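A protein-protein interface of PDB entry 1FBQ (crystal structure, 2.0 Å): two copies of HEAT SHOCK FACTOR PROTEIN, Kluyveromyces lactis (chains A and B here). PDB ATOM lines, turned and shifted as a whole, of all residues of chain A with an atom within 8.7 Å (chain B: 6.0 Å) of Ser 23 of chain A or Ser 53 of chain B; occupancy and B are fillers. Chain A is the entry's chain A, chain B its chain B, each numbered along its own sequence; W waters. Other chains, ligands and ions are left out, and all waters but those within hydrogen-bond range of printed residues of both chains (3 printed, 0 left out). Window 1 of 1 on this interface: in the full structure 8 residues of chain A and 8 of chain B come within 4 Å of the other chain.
The side-chain carboxylate (OE1) of Glu 17 of chain A is in salt-bridge range of the guanidinium group (NH2) of Arg 56 of chain B, 2.8 Å away.
A ring nitrogen (NE2) of His 21 of chain A lies close to the guanidinium group (NH2) of Arg 56 of chain B, 3.4 Å away.
The guanidinium group (NH1) of Arg 56 of chain B is in hydrogen-bond range of the backbone carbonyl oxygen (O) of Trp 22 of chain A (3.3 Å).
The side-chain hydroxyl (OG) of Ser 53 of chain B is in hydrogen-bond range of the backbone carbonyl oxygen (O) of Ser 23 of chain A (2.9 Å).
OG1 of Thr 24 of chain A is in hydrogen-bond range of NH1 of Arg 56 of chain B (3.1 Å).
The side-chain hydroxyl (OG) of Ser 53 of chain B is in hydrogen-bond range of the backbone carbonyl oxygen (O) of Gly 26 of chain A (3.4 Å).
The indole nitrogen (NE1) of Trp 22 of chain A is in hydrogen-bond range of the side-chain amide oxygen (OD1) of Asn 12 of chain A (2.8 Å).
A ring nitrogen (ND1) of His 21 of chain A sits at hydrogen-bond distance from the backbone carbonyl oxygen (O) of Glu 17 of chain A, at 3.1 Å.
O of His 21 of chain A lies within hydrogen-bond range of N of Val 30 of chain A (2.8 Å).
The side-chain hydroxyl (OG) of Ser 23 of chain A lies within hydrogen-bond range of the backbone carbonyl oxygen (O) of Ser 25 of chain A (2.4 Å).
The backbone carbonyl oxygen (O) of Ser 28 of chain A lies within hydrogen-bond range of the backbone NH (N) of Ser 23 of chain A (2.7 Å).
N of Ala 52 of chain B sits at hydrogen-bond distance from OD1 of Asn 50 of chain B, at 3.2 Å.
Arg 56 of chain B touches Lys 14 of chain A.
Trp 22 of chain A touches Asn 50 of chain B.
Trp 22 of chain A touches Ala 52 of chain B.
CB of Trp 22 of chain A touches OG of Ser 53 of chain B (3.8 Å).
Gln 57 of chain B touches Thr 24 of chain A (NE2 to CG2, 3.7 Å).
Gly 26 of chain A touches Ser 49 of chain B (O to CA, 3.9 Å).
Glu 27 of chain A touches Ser 49 of chain B (CG to C, 3.6 Å).
CB of Glu 27 of chain A touches ND2 of Asn 50 of chain B (3.7 Å).
Of the printed residues of chain B, Glu 17 of chain A touches Arg 56.
Ser 23 of chain A touches just one residue of chain B: Ser 53.
Of the printed residues of chain B, Thr 24 of chain A touches Arg 56 (3.1 Å) and Gln 57 (3.7 Å).
Printed residues of chain B within 4 Å of Gly 26 of chain A: Ser 49 and Ser 53.
Printed residues of chain B within 4 Å of Glu 27 of chain A: Ser 49 (3.6 Å) and Asn 50 (3.7 Å).
Val 30 of chain A touches none of the printed residues of chain B.
Of the printed residues of chain A, Ser 49 of chain B touches Gly 26 (3.9 Å) and Glu 27 (3.6 Å).
Phe 51 of chain B touches none of the printed residues of chain A.
Of the printed residues of chain A, Ala 52 of chain B touches Trp 22.
Ser 53 of chain B touches just these residues of chain A: Trp 22, Ser 23 and Gly 26.
The nearest printed residue of chain A that does not touch Ser 53 of chain B is Thr 24 of chain A (4.8 Å).
Of the 22 printed residues of chain A, 8 touch a printed residue of chain B.
Hydrophobic or aromatic side chains of chain A within 4 Å of the printed part of chain B: His 21 and Trp 22.
Of the 12 printed residues of chain B, 6 touch a printed residue of chain A.
Hydrophobic or aromatic side chains of chain B within 4 Å of the printed part of chain A: Ala 52.
Among the printed residues, 14 pairs touch across the chains.
No position is printed for both chains.
Water W1 lies within hydrogen-bond range of NH1 of Arg 56 of chain B (2.8 Å), O of Ser 23 of chain A (2.9 Å) and O of Ser 53 of chain B (3.1 Å).
Water W3 lies within hydrogen-bond range of the backbone carbonyl oxygen (O) of Ala 52 of chain B (2.8 Å) and the side-chain amino group (NZ) of Lys 14 of chain A (2.9 Å).
Water W2 bridges the side-chain carboxylate of Glu 27 of chain A (2.9 Å) and the side-chain amide nitrogen of Asn 50 of chain B (3.0 Å).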
ATOM      1  N   VAL A  11      25.478  27.059  25.939  1.00  0.00           N
ATOM      2  CA  VAL A  11      24.505  27.378  24.916  1.00  0.00           C
ATOM      3  C   VAL A  11      24.644  28.778  24.330  1.00  0.00           C
ATOM      4  O   VAL A  11      24.475  28.952  23.126  1.00  0.00           O
ATOM      5  CB  VAL A  11      23.047  27.179  25.441  1.00  0.00           C
ATOM      6  CG1 VAL A  11      22.040  27.610  24.358  1.00  0.00           C
ATOM      7  CG2 VAL A  11      22.834  25.693  25.814  1.00  0.00           C
ATOM      8  N   ASN A  12      24.940  29.768  25.164  1.00  0.00           N
ATOM      9  CA  ASN A  12      25.047  31.117  24.643  1.00  0.00           C
ATOM     10  C   ASN A  12      26.458  31.528  24.178  1.00  0.00           C
ATOM     11  O   ASN A  12      26.740  32.713  24.006  1.00  0.00           O
ATOM     12  CB  ASN A  12      24.460  32.139  25.638  1.00  0.00           C
ATOM     13  CG  ASN A  12      22.942  31.940  25.859  1.00  0.00           C
ATOM     14  OD1 ASN A  12      22.196  31.601  24.913  1.00  0.00           O
ATOM     15  ND2 ASN A  12      22.481  32.162  27.098  1.00  0.00           N
ATOM     16  N   LYS A  14      28.629  31.445  21.048  1.00  0.00           N
ATOM     17  CA  LYS A  14      28.484  31.254  19.596  1.00  0.00           C
ATOM     18  C   LYS A  14      29.382  30.169  19.016  1.00  0.00           C
ATOM     19  O   LYS A  14      29.072  29.565  17.993  1.00  0.00           O
ATOM     20  CB  LYS A  14      28.781  32.574  18.853  1.00  0.00           C
ATOM     21  CG  LYS A  14      28.028  33.818  19.373  1.00  0.00           C
ATOM     22  CD  LYS A  14      26.522  33.829  18.975  1.00  0.00           C
ATOM     23  CE  LYS A  14      25.688  34.921  19.716  1.00  0.00           C
ATOM     24  NZ  LYS A  14      24.194  34.737  19.469  1.00  0.00           N
ATOM     25  N   GLU A  17      27.728  26.784  18.346  1.00  0.00           N
ATOM     26  CA  GLU A  17      26.630  26.822  17.369  1.00  0.00           C
ATOM     27  C   GLU A  17      26.325  25.546  16.555  1.00  0.00           C
ATOM     28  O   GLU A  17      25.163  25.172  16.390  1.00  0.00           O
ATOM     29  CB  GLU A  17      26.865  28.020  16.425  1.00  0.00           C
ATOM     30  CG  GLU A  17      25.963  28.071  15.195  1.00  0.00           C
ATOM     31  CD  GLU A  17      24.484  28.254  15.530  1.00  0.00           C
ATOM     32  OE1 GLU A  17      23.657  27.821  14.723  1.00  0.00           O
ATOM     33  OE2 GLU A  17      24.130  28.843  16.578  1.00  0.00           O
ATOM     34  N   ILE A  20      25.014  22.839  19.603  1.00  0.00           N
ATOM     35  CA  ILE A  20      23.889  23.145  20.472  1.00  0.00           C
ATOM     36  C   ILE A  20      23.551  24.630  20.250  1.00  0.00           C
ATOM     37  O   ILE A  20      24.456  25.467  20.158  1.00  0.00           O
ATOM     38  CB  ILE A  20      24.273  22.814  21.925  1.00  0.00           C
ATOM     39  CG1 ILE A  20      23.093  23.064  22.846  1.00  0.00           C
ATOM     40  CG2 ILE A  20      25.544  23.611  22.331  1.00  0.00           C
ATOM     41  CD1 ILE A  20      23.232  22.370  24.194  1.00  0.00           C
ATOM     42  N   HIS A  21      22.263  24.960  20.116  1.00  0.00           N
ATOM     43  CA  HIS A  21      21.878  26.350  19.864  1.00  0.00           C
ATOM     44  C   HIS A  21      20.383  26.590  20.054  1.00  0.00           C
ATOM     45  O   HIS A  21      19.592  25.652  19.995  1.00  0.00           O
ATOM     46  CB  HIS A  21      22.263  26.770  18.439  1.00  0.00           C
ATOM     47  CG  HIS A  21      21.518  26.037  17.364  1.00  0.00           C
ATOM     48  ND1 HIS A  21      22.092  25.051  16.599  1.00  0.00           N
ATOM     49  CD2 HIS A  21      20.233  26.132  16.949  1.00  0.00           C
ATOM     50  CE1 HIS A  21      21.193  24.567  15.758  1.00  0.00           C
ATOM     51  NE2 HIS A  21      20.054  25.206  15.953  1.00  0.00           N
ATOM     52  N   TRP A  22      20.009  27.843  20.308  1.00  0.00           N
ATOM     53  CA  TRP A  22      18.595  28.174  20.452  1.00  0.00           C
ATOM     54  C   TRP A  22      17.970  27.899  19.095  1.00  0.00           C
ATOM     55  O   TRP A  22      18.595  28.083  18.061  1.00  0.00           O
ATOM     56  CB  TRP A  22      18.394  29.652  20.796  1.00  0.00           C
ATOM     57  CG  TRP A  22      18.665  29.990  22.239  1.00  0.00           C
ATOM     58  CD1 TRP A  22      19.805  30.524  22.756  1.00  0.00           C
ATOM     59  CD2 TRP A  22      17.809  29.724  23.350  1.00  0.00           C
ATOM     60  NE1 TRP A  22      19.722  30.597  24.115  1.00  0.00           N
ATOM     61  CE2 TRP A  22      18.504  30.112  24.512  1.00  0.00           C
ATOM     62  CE3 TRP A  22      16.516  29.189  23.478  1.00  0.00           C
ATOM     63  CZ2 TRP A  22      17.962  29.985  25.788  1.00  0.00           C
ATOM     64  CZ3 TRP A  22      15.971  29.061  24.757  1.00  0.00           C
ATOM     65  CH2 TRP A  22      16.703  29.461  25.899  1.00  0.00           C
ATOM     66  N   SER A  23      16.721  27.484  19.113  1.00  0.00           N
ATOM     67  CA  SER A  23      15.979  27.171  17.907  1.00  0.00           C
ATOM     68  C   SER A  23      15.770  28.398  17.041  1.00  0.00           C
ATOM     69  O   SER A  23      15.639  29.511  17.561  1.00  0.00           O
ATOM     70  CB  SER A  23      14.627  26.618  18.304  1.00  0.00           C
ATOM     71  OG  SER A  23      13.753  26.625  17.201  1.00  0.00           O
ATOM     72  N   THR A  24      15.755  28.186  15.723  1.00  0.00           N
ATOM     73  CA  THR A  24      15.516  29.262  14.764  1.00  0.00           C
ATOM     74  C   THR A  24      14.062  29.702  14.979  1.00  0.00           C
ATOM     75  O   THR A  24      13.766  30.889  15.127  1.00  0.00           O
ATOM     76  CB  THR A  24      15.669  28.759  13.316  1.00  0.00           C
ATOM     77  OG1 THR A  24      17.049  28.438  13.065  1.00  0.00           O
ATOM     78  CG2 THR A  24      15.184  29.829  12.315  1.00  0.00           C
ATOM     79  N   SER A  25      13.160  28.734  15.029  1.00  0.00           N
ATOM     80  CA  SER A  25      11.742  29.026  15.253  1.00  0.00           C
ATOM     81  C   SER A  25      11.295  28.344  16.538  1.00  0.00           C
ATOM     82  O   SER A  25      11.439  27.138  16.716  1.00  0.00           O
ATOM     83  CB  SER A  25      10.904  28.547  14.059  1.00  0.00           C
ATOM     84  OG  SER A  25      11.143  27.174  13.773  1.00  0.00           O
ATOM     85  N   GLY A  26      10.767  29.123  17.462  1.00  0.00           N
ATOM     86  CA  GLY A  26      10.368  28.529  18.714  1.00  0.00           C
ATOM     87  C   GLY A  26      11.315  29.058  19.768  1.00  0.00           C
ATOM     88  O   GLY A  26      12.197  29.890  19.481  1.00  0.00           O
ATOM     89  N   GLU A  27      11.126  28.576  20.981  1.00  0.00           N
ATOM     90  CA  GLU A  27      11.912  28.998  22.123  1.00  0.00           C
ATOM     91  C   GLU A  27      12.528  27.759  22.727  1.00  0.00           C
ATOM     92  O   GLU A  27      12.317  27.486  23.903  1.00  0.00           O
ATOM     93  CB  GLU A  27      10.984  29.602  23.162  1.00  0.00           C
ATOM     94  CG  GLU A  27      10.433  30.929  22.771  1.00  0.00           C
ATOM     95  CD  GLU A  27       9.048  31.130  23.295  1.00  0.00           C
ATOM     96  OE1 GLU A  27       8.091  30.743  22.588  1.00  0.00           O
ATOM     97  OE2 GLU A  27       8.916  31.657  24.414  1.00  0.00           O
ATOM     98  N   SER A  28      13.256  26.990  21.946  1.00  0.00           N
ATOM     99  CA  SER A  28      13.829  25.787  22.503  1.00  0.00           C
ATOM    100  C   SER A  28      15.329  25.686  22.245  1.00  0.00           C
ATOM    101  O   SER A  28      15.900  26.403  21.435  1.00  0.00           O
ATOM    102  CB  SER A  28      13.081  24.570  21.930  1.00  0.00           C
ATOM    103  OG  SER A  28      13.362  24.408  20.553  1.00  0.00           O
ATOM    104  N   ILE A  29      15.953  24.781  22.975  1.00  0.00           N
ATOM    105  CA  ILE A  29      17.368  24.513  22.862  1.00  0.00           C
ATOM    106  C   ILE A  29      17.448  23.255  22.013  1.00  0.00           C
ATOM    107  O   ILE A  29      16.842  22.242  22.333  1.00  0.00           O
ATOM    108  CB  ILE A  29      17.978  24.249  24.234  1.00  0.00           C
ATOM    109  CG1 ILE A  29      17.929  25.539  25.056  1.00  0.00           C
ATOM    110  CG2 ILE A  29      19.399  23.734  24.069  1.00  0.00           C
ATOM    111  CD1 ILE A  29      18.278  25.322  26.551  1.00  0.00           C
ATOM    112  N   VAL A  30      18.235  23.346  20.953  1.00  0.00           N
ATOM    113  CA  VAL A  30      18.362  22.296  19.975  1.00  0.00           C
ATOM    114  C   VAL A  30      19.756  21.672  19.981  1.00  0.00           C
ATOM    115  O   VAL A  30      20.772  22.382  20.017  1.00  0.00           O
ATOM    116  CB  VAL A  30      18.086  22.927  18.544  1.00  0.00           C
ATOM    117  CG1 VAL A  30      18.313  21.923  17.444  1.00  0.00           C
ATOM    118  CG2 VAL A  30      16.669  23.524  18.481  1.00  0.00           C
ATOM    119  N   VAL A  31      19.792  20.335  19.971  1.00  0.00           N
ATOM    120  CA  VAL A  31      21.033  19.579  19.864  1.00  0.00           C
ATOM    121  C   VAL A  31      20.779  18.794  18.568  1.00  0.00           C
ATOM    122  O   VAL A  31      20.165  17.725  18.576  1.00  0.00           O
ATOM    123  CB  VAL A  31      21.266  18.624  21.057  1.00  0.00           C
ATOM    124  CG1 VAL A  31      22.461  17.664  20.753  1.00  0.00           C
ATOM    125  CG2 VAL A  31      21.606  19.455  22.312  1.00  0.00           C
ATOM    126  N   TRP A  63      13.955  21.820  32.066  1.00  0.00           N
ATOM    127  CA  TRP A  63      14.027  21.619  30.625  1.00  0.00           C
ATOM    128  C   TRP A  63      13.683  20.186  30.228  1.00  0.00           C
ATOM    129  O   TRP A  63      14.263  19.228  30.757  1.00  0.00           O
ATOM    130  CB  TRP A  63      15.412  22.020  30.131  1.00  0.00           C
ATOM    131  CG  TRP A  63      15.576  23.503  30.211  1.00  0.00           C
ATOM    132  CD1 TRP A  63      15.943  24.245  31.314  1.00  0.00           C
ATOM    133  CD2 TRP A  63      15.257  24.448  29.184  1.00  0.00           C
ATOM    134  NE1 TRP A  63      15.867  25.596  31.024  1.00  0.00           N
ATOM    135  CE2 TRP A  63      15.454  25.748  29.727  1.00  0.00           C
ATOM    136  CE3 TRP A  63      14.825  24.326  27.859  1.00  0.00           C
ATOM    137  CZ2 TRP A  63      15.241  26.908  28.989  1.00  0.00           C
ATOM    138  CZ3 TRP A  63      14.610  25.485  27.117  1.00  0.00           C
ATOM    139  CH2 TRP A  63      14.821  26.763  27.688  1.00  0.00           C
ATOM    140  N   VAL A  66      11.302  17.858  23.724  1.00  0.00           N
ATOM    141  CA  VAL A  66      10.111  18.202  22.986  1.00  0.00           C
ATOM    142  C   VAL A  66       9.570  16.998  22.231  1.00  0.00           C
ATOM    143  O   VAL A  66      10.343  16.247  21.601  1.00  0.00           O
ATOM    144  CB  VAL A  66      10.410  19.332  21.976  1.00  0.00           C
ATOM    145  CG1 VAL A  66       9.211  19.525  21.001  1.00  0.00           C
ATOM    146  CG2 VAL A  66      10.688  20.612  22.737  1.00  0.00           C
ATOM    147  N   ARG A  81      18.570  13.841  17.012  1.00  0.00           N
ATOM    148  CA  ARG A  81      18.165  15.265  17.103  1.00  0.00           C
ATOM    149  C   ARG A  81      17.314  15.414  18.359  1.00  0.00           C
ATOM    150  O   ARG A  81      16.289  14.760  18.471  1.00  0.00           O
ATOM    151  CB  ARG A  81      17.307  15.730  15.903  1.00  0.00           C
ATOM    152  CG  ARG A  81      16.960  17.242  15.967  1.00  0.00           C
ATOM    153  CD  ARG A  81      16.087  17.732  14.790  1.00  0.00           C
ATOM    154  NE  ARG A  81      15.765  19.179  14.857  1.00  0.00           N
ATOM    155  CZ  ARG A  81      16.576  20.166  14.467  1.00  0.00           C
ATOM    156  NH1 ARG A  81      17.801  19.918  13.952  1.00  0.00           N
ATOM    157  NH2 ARG A  81      16.170  21.419  14.605  1.00  0.00           N
ATOM    158  N   TRP A  82      17.727  16.286  19.277  1.00  0.00           N
ATOM    159  CA  TRP A  82      17.008  16.529  20.510  1.00  0.00           C
ATOM    160  C   TRP A  82      16.723  18.032  20.656  1.00  0.00           C
ATOM    161  O   TRP A  82      17.592  18.870  20.415  1.00  0.00           O
ATOM    162  CB  TRP A  82      17.851  16.096  21.711  1.00  0.00           C
ATOM    163  CG  TRP A  82      17.933  14.578  21.909  1.00  0.00           C
ATOM    164  CD1 TRP A  82      18.439  13.662  21.048  1.00  0.00           C
ATOM    165  CD2 TRP A  82      17.429  13.852  23.027  1.00  0.00           C
ATOM    166  NE1 TRP A  82      18.283  12.380  21.559  1.00  0.00           N
ATOM    167  CE2 TRP A  82      17.659  12.472  22.775  1.00  0.00           C
ATOM    168  CE3 TRP A  82      16.797  14.230  24.217  1.00  0.00           C
ATOM    169  CZ2 TRP A  82      17.280  11.475  23.664  1.00  0.00           C
ATOM    170  CZ3 TRP A  82      16.414  13.241  25.107  1.00  0.00           C
ATOM    171  CH2 TRP A  82      16.660  11.870  24.827  1.00  0.00           C
ATOM    172  N   GLU A  83      15.514  18.358  21.079  1.00  0.00           N
ATOM    173  CA  GLU A  83      15.124  19.741  21.290  1.00  0.00           C
ATOM    174  C   GLU A  83      14.486  19.758  22.671  1.00  0.00           C
ATOM    175  O   GLU A  83      13.668  18.891  22.978  1.00  0.00           O
ATOM    176  CB  GLU A  83      14.117  20.113  20.220  1.00  0.00           C
ATOM    177  CG  GLU A  83      13.902  21.571  20.003  1.00  0.00           C
ATOM    178  CD  GLU A  83      12.826  21.783  18.964  1.00  0.00           C
ATOM    179  OE1 GLU A  83      12.877  21.040  17.936  1.00  0.00           O
ATOM    180  OE2 GLU A  83      11.943  22.663  19.194  1.00  0.00           O
ATOM    181  N   PHE A  84      14.848  20.741  23.494  1.00  0.00           N
ATOM    182  CA  PHE A  84      14.328  20.842  24.854  1.00  0.00           C
ATOM    183  C   PHE A  84      13.583  22.163  25.053  1.00  0.00           C
ATOM    184  O   PHE A  84      14.009  23.210  24.538  1.00  0.00           O
ATOM    185  CB  PHE A  84      15.478  20.796  25.874  1.00  0.00           C
ATOM    186  CG  PHE A  84      16.386  19.569  25.747  1.00  0.00           C
ATOM    187  CD1 PHE A  84      16.091  18.393  26.439  1.00  0.00           C
ATOM    188  CD2 PHE A  84      17.547  19.622  24.974  1.00  0.00           C
ATOM    189  CE1 PHE A  84      16.939  17.286  26.376  1.00  0.00           C
ATOM    190  CE2 PHE A  84      18.421  18.506  24.893  1.00  0.00           C
ATOM    191  CZ  PHE A  84      18.111  17.338  25.600  1.00  0.00           C
ATOM    192  N   PHE B   3      13.441  36.104   7.667  1.00  0.00           N
ATOM    193  CA  PHE B   3      13.859  36.846   8.847  1.00  0.00           C
ATOM    194  C   PHE B   3      14.059  38.311   8.497  1.00  0.00           C
ATOM    195  O   PHE B   3      13.526  39.197   9.157  1.00  0.00           O
ATOM    196  CB  PHE B   3      15.188  36.337   9.396  1.00  0.00           C
ATOM    197  CG  PHE B   3      15.675  37.120  10.586  1.00  0.00           C
ATOM    198  CD1 PHE B   3      15.040  36.998  11.821  1.00  0.00           C
ATOM    199  CD2 PHE B   3      16.734  38.019  10.460  1.00  0.00           C
ATOM    200  CE1 PHE B   3      15.449  37.765  12.924  1.00  0.00           C
ATOM    201  CE2 PHE B   3      17.153  38.792  11.550  1.00  0.00           C
ATOM    202  CZ  PHE B   3      16.512  38.668  12.786  1.00  0.00           C
ATOM    203  N   SER B  49       9.121  33.229  19.910  1.00  0.00           N
ATOM    204  CA  SER B  49      10.555  33.388  19.709  1.00  0.00           C
ATOM    205  C   SER B  49      10.964  34.043  21.011  1.00  0.00           C
ATOM    206  O   SER B  49      10.104  34.501  21.740  1.00  0.00           O
ATOM    207  CB  SER B  49      10.838  34.342  18.560  1.00  0.00           C
ATOM    208  OG  SER B  49      12.234  34.513  18.396  1.00  0.00           O
ATOM    209  N   ASN B  50      12.250  34.056  21.332  1.00  0.00           N
ATOM    210  CA  ASN B  50      12.681  34.737  22.539  1.00  0.00           C
ATOM    211  C   ASN B  50      13.869  35.603  22.158  1.00  0.00           C
ATOM    212  O   ASN B  50      14.319  35.598  21.000  1.00  0.00           O
ATOM    213  CB  ASN B  50      13.035  33.770  23.668  1.00  0.00           C
ATOM    214  CG  ASN B  50      14.149  32.801  23.310  1.00  0.00           C
ATOM    215  OD1 ASN B  50      15.089  33.143  22.594  1.00  0.00           O
ATOM    216  ND2 ASN B  50      14.061  31.564  23.863  1.00  0.00           N
ATOM    217  N   PHE B  51      14.385  36.353  23.120  1.00  0.00           N
ATOM    218  CA  PHE B  51      15.484  37.256  22.798  1.00  0.00           C
ATOM    219  C   PHE B  51      16.751  36.619  22.213  1.00  0.00           C
ATOM    220  O   PHE B  51      17.304  37.065  21.184  1.00  0.00           O
ATOM    221  CB  PHE B  51      15.845  38.095  24.006  1.00  0.00           C
ATOM    222  CG  PHE B  51      16.648  39.274  23.648  1.00  0.00           C
ATOM    223  CD1 PHE B  51      16.077  40.308  22.899  1.00  0.00           C
ATOM    224  CD2 PHE B  51      17.985  39.380  24.065  1.00  0.00           C
ATOM    225  CE1 PHE B  51      16.830  41.451  22.568  1.00  0.00           C
ATOM    226  CE2 PHE B  51      18.732  40.521  23.747  1.00  0.00           C
ATOM    227  CZ  PHE B  51      18.159  41.553  23.000  1.00  0.00           C
ATOM    228  N   ALA B  52      17.190  35.555  22.851  1.00  0.00           N
ATOM    229  CA  ALA B  52      18.395  34.867  22.426  1.00  0.00           C
ATOM    230  C   ALA B  52      18.212  34.331  21.009  1.00  0.00           C
ATOM    231  O   ALA B  52      19.138  34.375  20.236  1.00  0.00           O
ATOM    232  CB  ALA B  52      18.720  33.719  23.442  1.00  0.00           C
ATOM    233  N   SER B  53      17.023  33.819  20.687  1.00  0.00           N
ATOM    234  CA  SER B  53      16.699  33.313  19.323  1.00  0.00           C
ATOM    235  C   SER B  53      16.805  34.447  18.311  1.00  0.00           C
ATOM    236  O   SER B  53      17.328  34.299  17.204  1.00  0.00           O
ATOM    237  CB  SER B  53      15.257  32.783  19.243  1.00  0.00           C
ATOM    238  OG  SER B  53      15.201  31.435  19.668  1.00  0.00           O
ATOM    239  N   PHE B  54      16.263  35.581  18.700  1.00  0.00           N
ATOM    240  CA  PHE B  54      16.290  36.765  17.855  1.00  0.00           C
ATOM    241  C   PHE B  54      17.732  37.187  17.601  1.00  0.00           C
ATOM    242  O   PHE B  54      18.147  37.422  16.445  1.00  0.00           O
ATOM    243  CB  PHE B  54      15.513  37.879  18.541  1.00  0.00           C
ATOM    244  CG  PHE B  54      15.550  39.200  17.800  1.00  0.00           C
ATOM    245  CD1 PHE B  54      15.038  39.301  16.512  1.00  0.00           C
ATOM    246  CD2 PHE B  54      16.094  40.325  18.399  1.00  0.00           C
ATOM    247  CE1 PHE B  54      15.062  40.501  15.816  1.00  0.00           C
ATOM    248  CE2 PHE B  54      16.130  41.530  17.723  1.00  0.00           C
ATOM    249  CZ  PHE B  54      15.606  41.617  16.413  1.00  0.00           C
ATOM    250  N   VAL B  55      18.519  37.241  18.673  1.00  0.00           N
ATOM    251  CA  VAL B  55      19.892  37.674  18.558  1.00  0.00           C
ATOM    252  C   VAL B  55      20.732  36.702  17.730  1.00  0.00           C
ATOM    253  O   VAL B  55      21.593  37.125  16.951  1.00  0.00           O
ATOM    254  CB  VAL B  55      20.500  37.926  19.952  1.00  0.00           C
ATOM    255  CG1 VAL B  55      21.971  38.264  19.804  1.00  0.00           C
ATOM    256  CG2 VAL B  55      19.773  39.123  20.637  1.00  0.00           C
ATOM    257  N   ARG B  56      20.471  35.400  17.875  1.00  0.00           N
ATOM    258  CA  ARG B  56      21.189  34.419  17.084  1.00  0.00           C
ATOM    259  C   ARG B  56      20.910  34.688  15.608  1.00  0.00           C
ATOM    260  O   ARG B  56      21.786  34.567  14.784  1.00  0.00           O
ATOM    261  CB  ARG B  56      20.753  32.992  17.448  1.00  0.00           C
ATOM    262  CG  ARG B  56      21.205  31.941  16.445  1.00  0.00           C
ATOM    263  CD  ARG B  56      20.986  30.514  17.014  1.00  0.00           C
ATOM    264  NE  ARG B  56      21.294  29.458  16.053  1.00  0.00           N
ATOM    265  CZ  ARG B  56      20.443  28.973  15.161  1.00  0.00           C
ATOM    266  NH1 ARG B  56      19.198  29.430  15.094  1.00  0.00           N
ATOM    267  NH2 ARG B  56      20.853  28.036  14.302  1.00  0.00           N
ATOM    268  N   GLN B  57      19.689  35.062  15.264  1.00  0.00           N
ATOM    269  CA  GLN B  57      19.384  35.350  13.844  1.00  0.00           C
ATOM    270  C   GLN B  57      20.107  36.604  13.358  1.00  0.00           C
ATOM    271  O   GLN B  57      20.678  36.634  12.261  1.00  0.00           O
ATOM    272  CB  GLN B  57      17.902  35.551  13.680  1.00  0.00           C
ATOM    273  CG  GLN B  57      17.153  34.442  14.282  1.00  0.00           C
ATOM    274  CD  GLN B  57      16.738  33.465  13.274  1.00  0.00           C
ATOM    275  OE1 GLN B  57      15.635  33.578  12.691  1.00  0.00           O
ATOM    276  NE2 GLN B  57      17.607  32.479  13.018  1.00  0.00           N
ATOM    277  N   LEU B  58      20.075  37.641  14.175  1.00  0.00           N
ATOM    278  CA  LEU B  58      20.743  38.896  13.845  1.00  0.00           C
ATOM    279  C   LEU B  58      22.203  38.598  13.545  1.00  0.00           C
ATOM    280  O   LEU B  58      22.794  39.145  12.585  1.00  0.00           O
ATOM    281  CB  LEU B  58      20.659  39.872  15.037  1.00  0.00           C
ATOM    282  CG  LEU B  58      19.342  40.617  15.327  1.00  0.00           C
ATOM    283  CD1 LEU B  58      19.503  41.565  16.575  1.00  0.00           C
ATOM    284  CD2 LEU B  58      18.946  41.454  14.085  1.00  0.00           C
ATOM    285  N   MET B  60      23.506  35.844  12.427  1.00  0.00           N
ATOM    286  CA  MET B  60      23.640  35.170  11.135  1.00  0.00           C
ATOM    287  C   MET B  60      23.562  36.153   9.961  1.00  0.00           C
ATOM    288  O   MET B  60      24.048  35.872   8.849  1.00  0.00           O
ATOM    289  CB  MET B  60      22.557  34.109  10.982  1.00  0.00           C
ATOM    290  CG  MET B  60      22.700  32.937  11.939  1.00  0.00           C
ATOM    291  SD  MET B  60      21.589  31.608  11.486  1.00  0.00           S
ATOM    292  CE  MET B  60      20.371  31.619  12.872  1.00  0.00           C
HETATM  293  O   HOH W   1      17.733  31.303  16.578  1.00  0.00           O
HETATM  294  O   HOH W   2      11.562  31.431  25.494  1.00  0.00           O
HETATM  295  O   HOH W   3      21.835  34.353  21.103  1.00  0.00           O
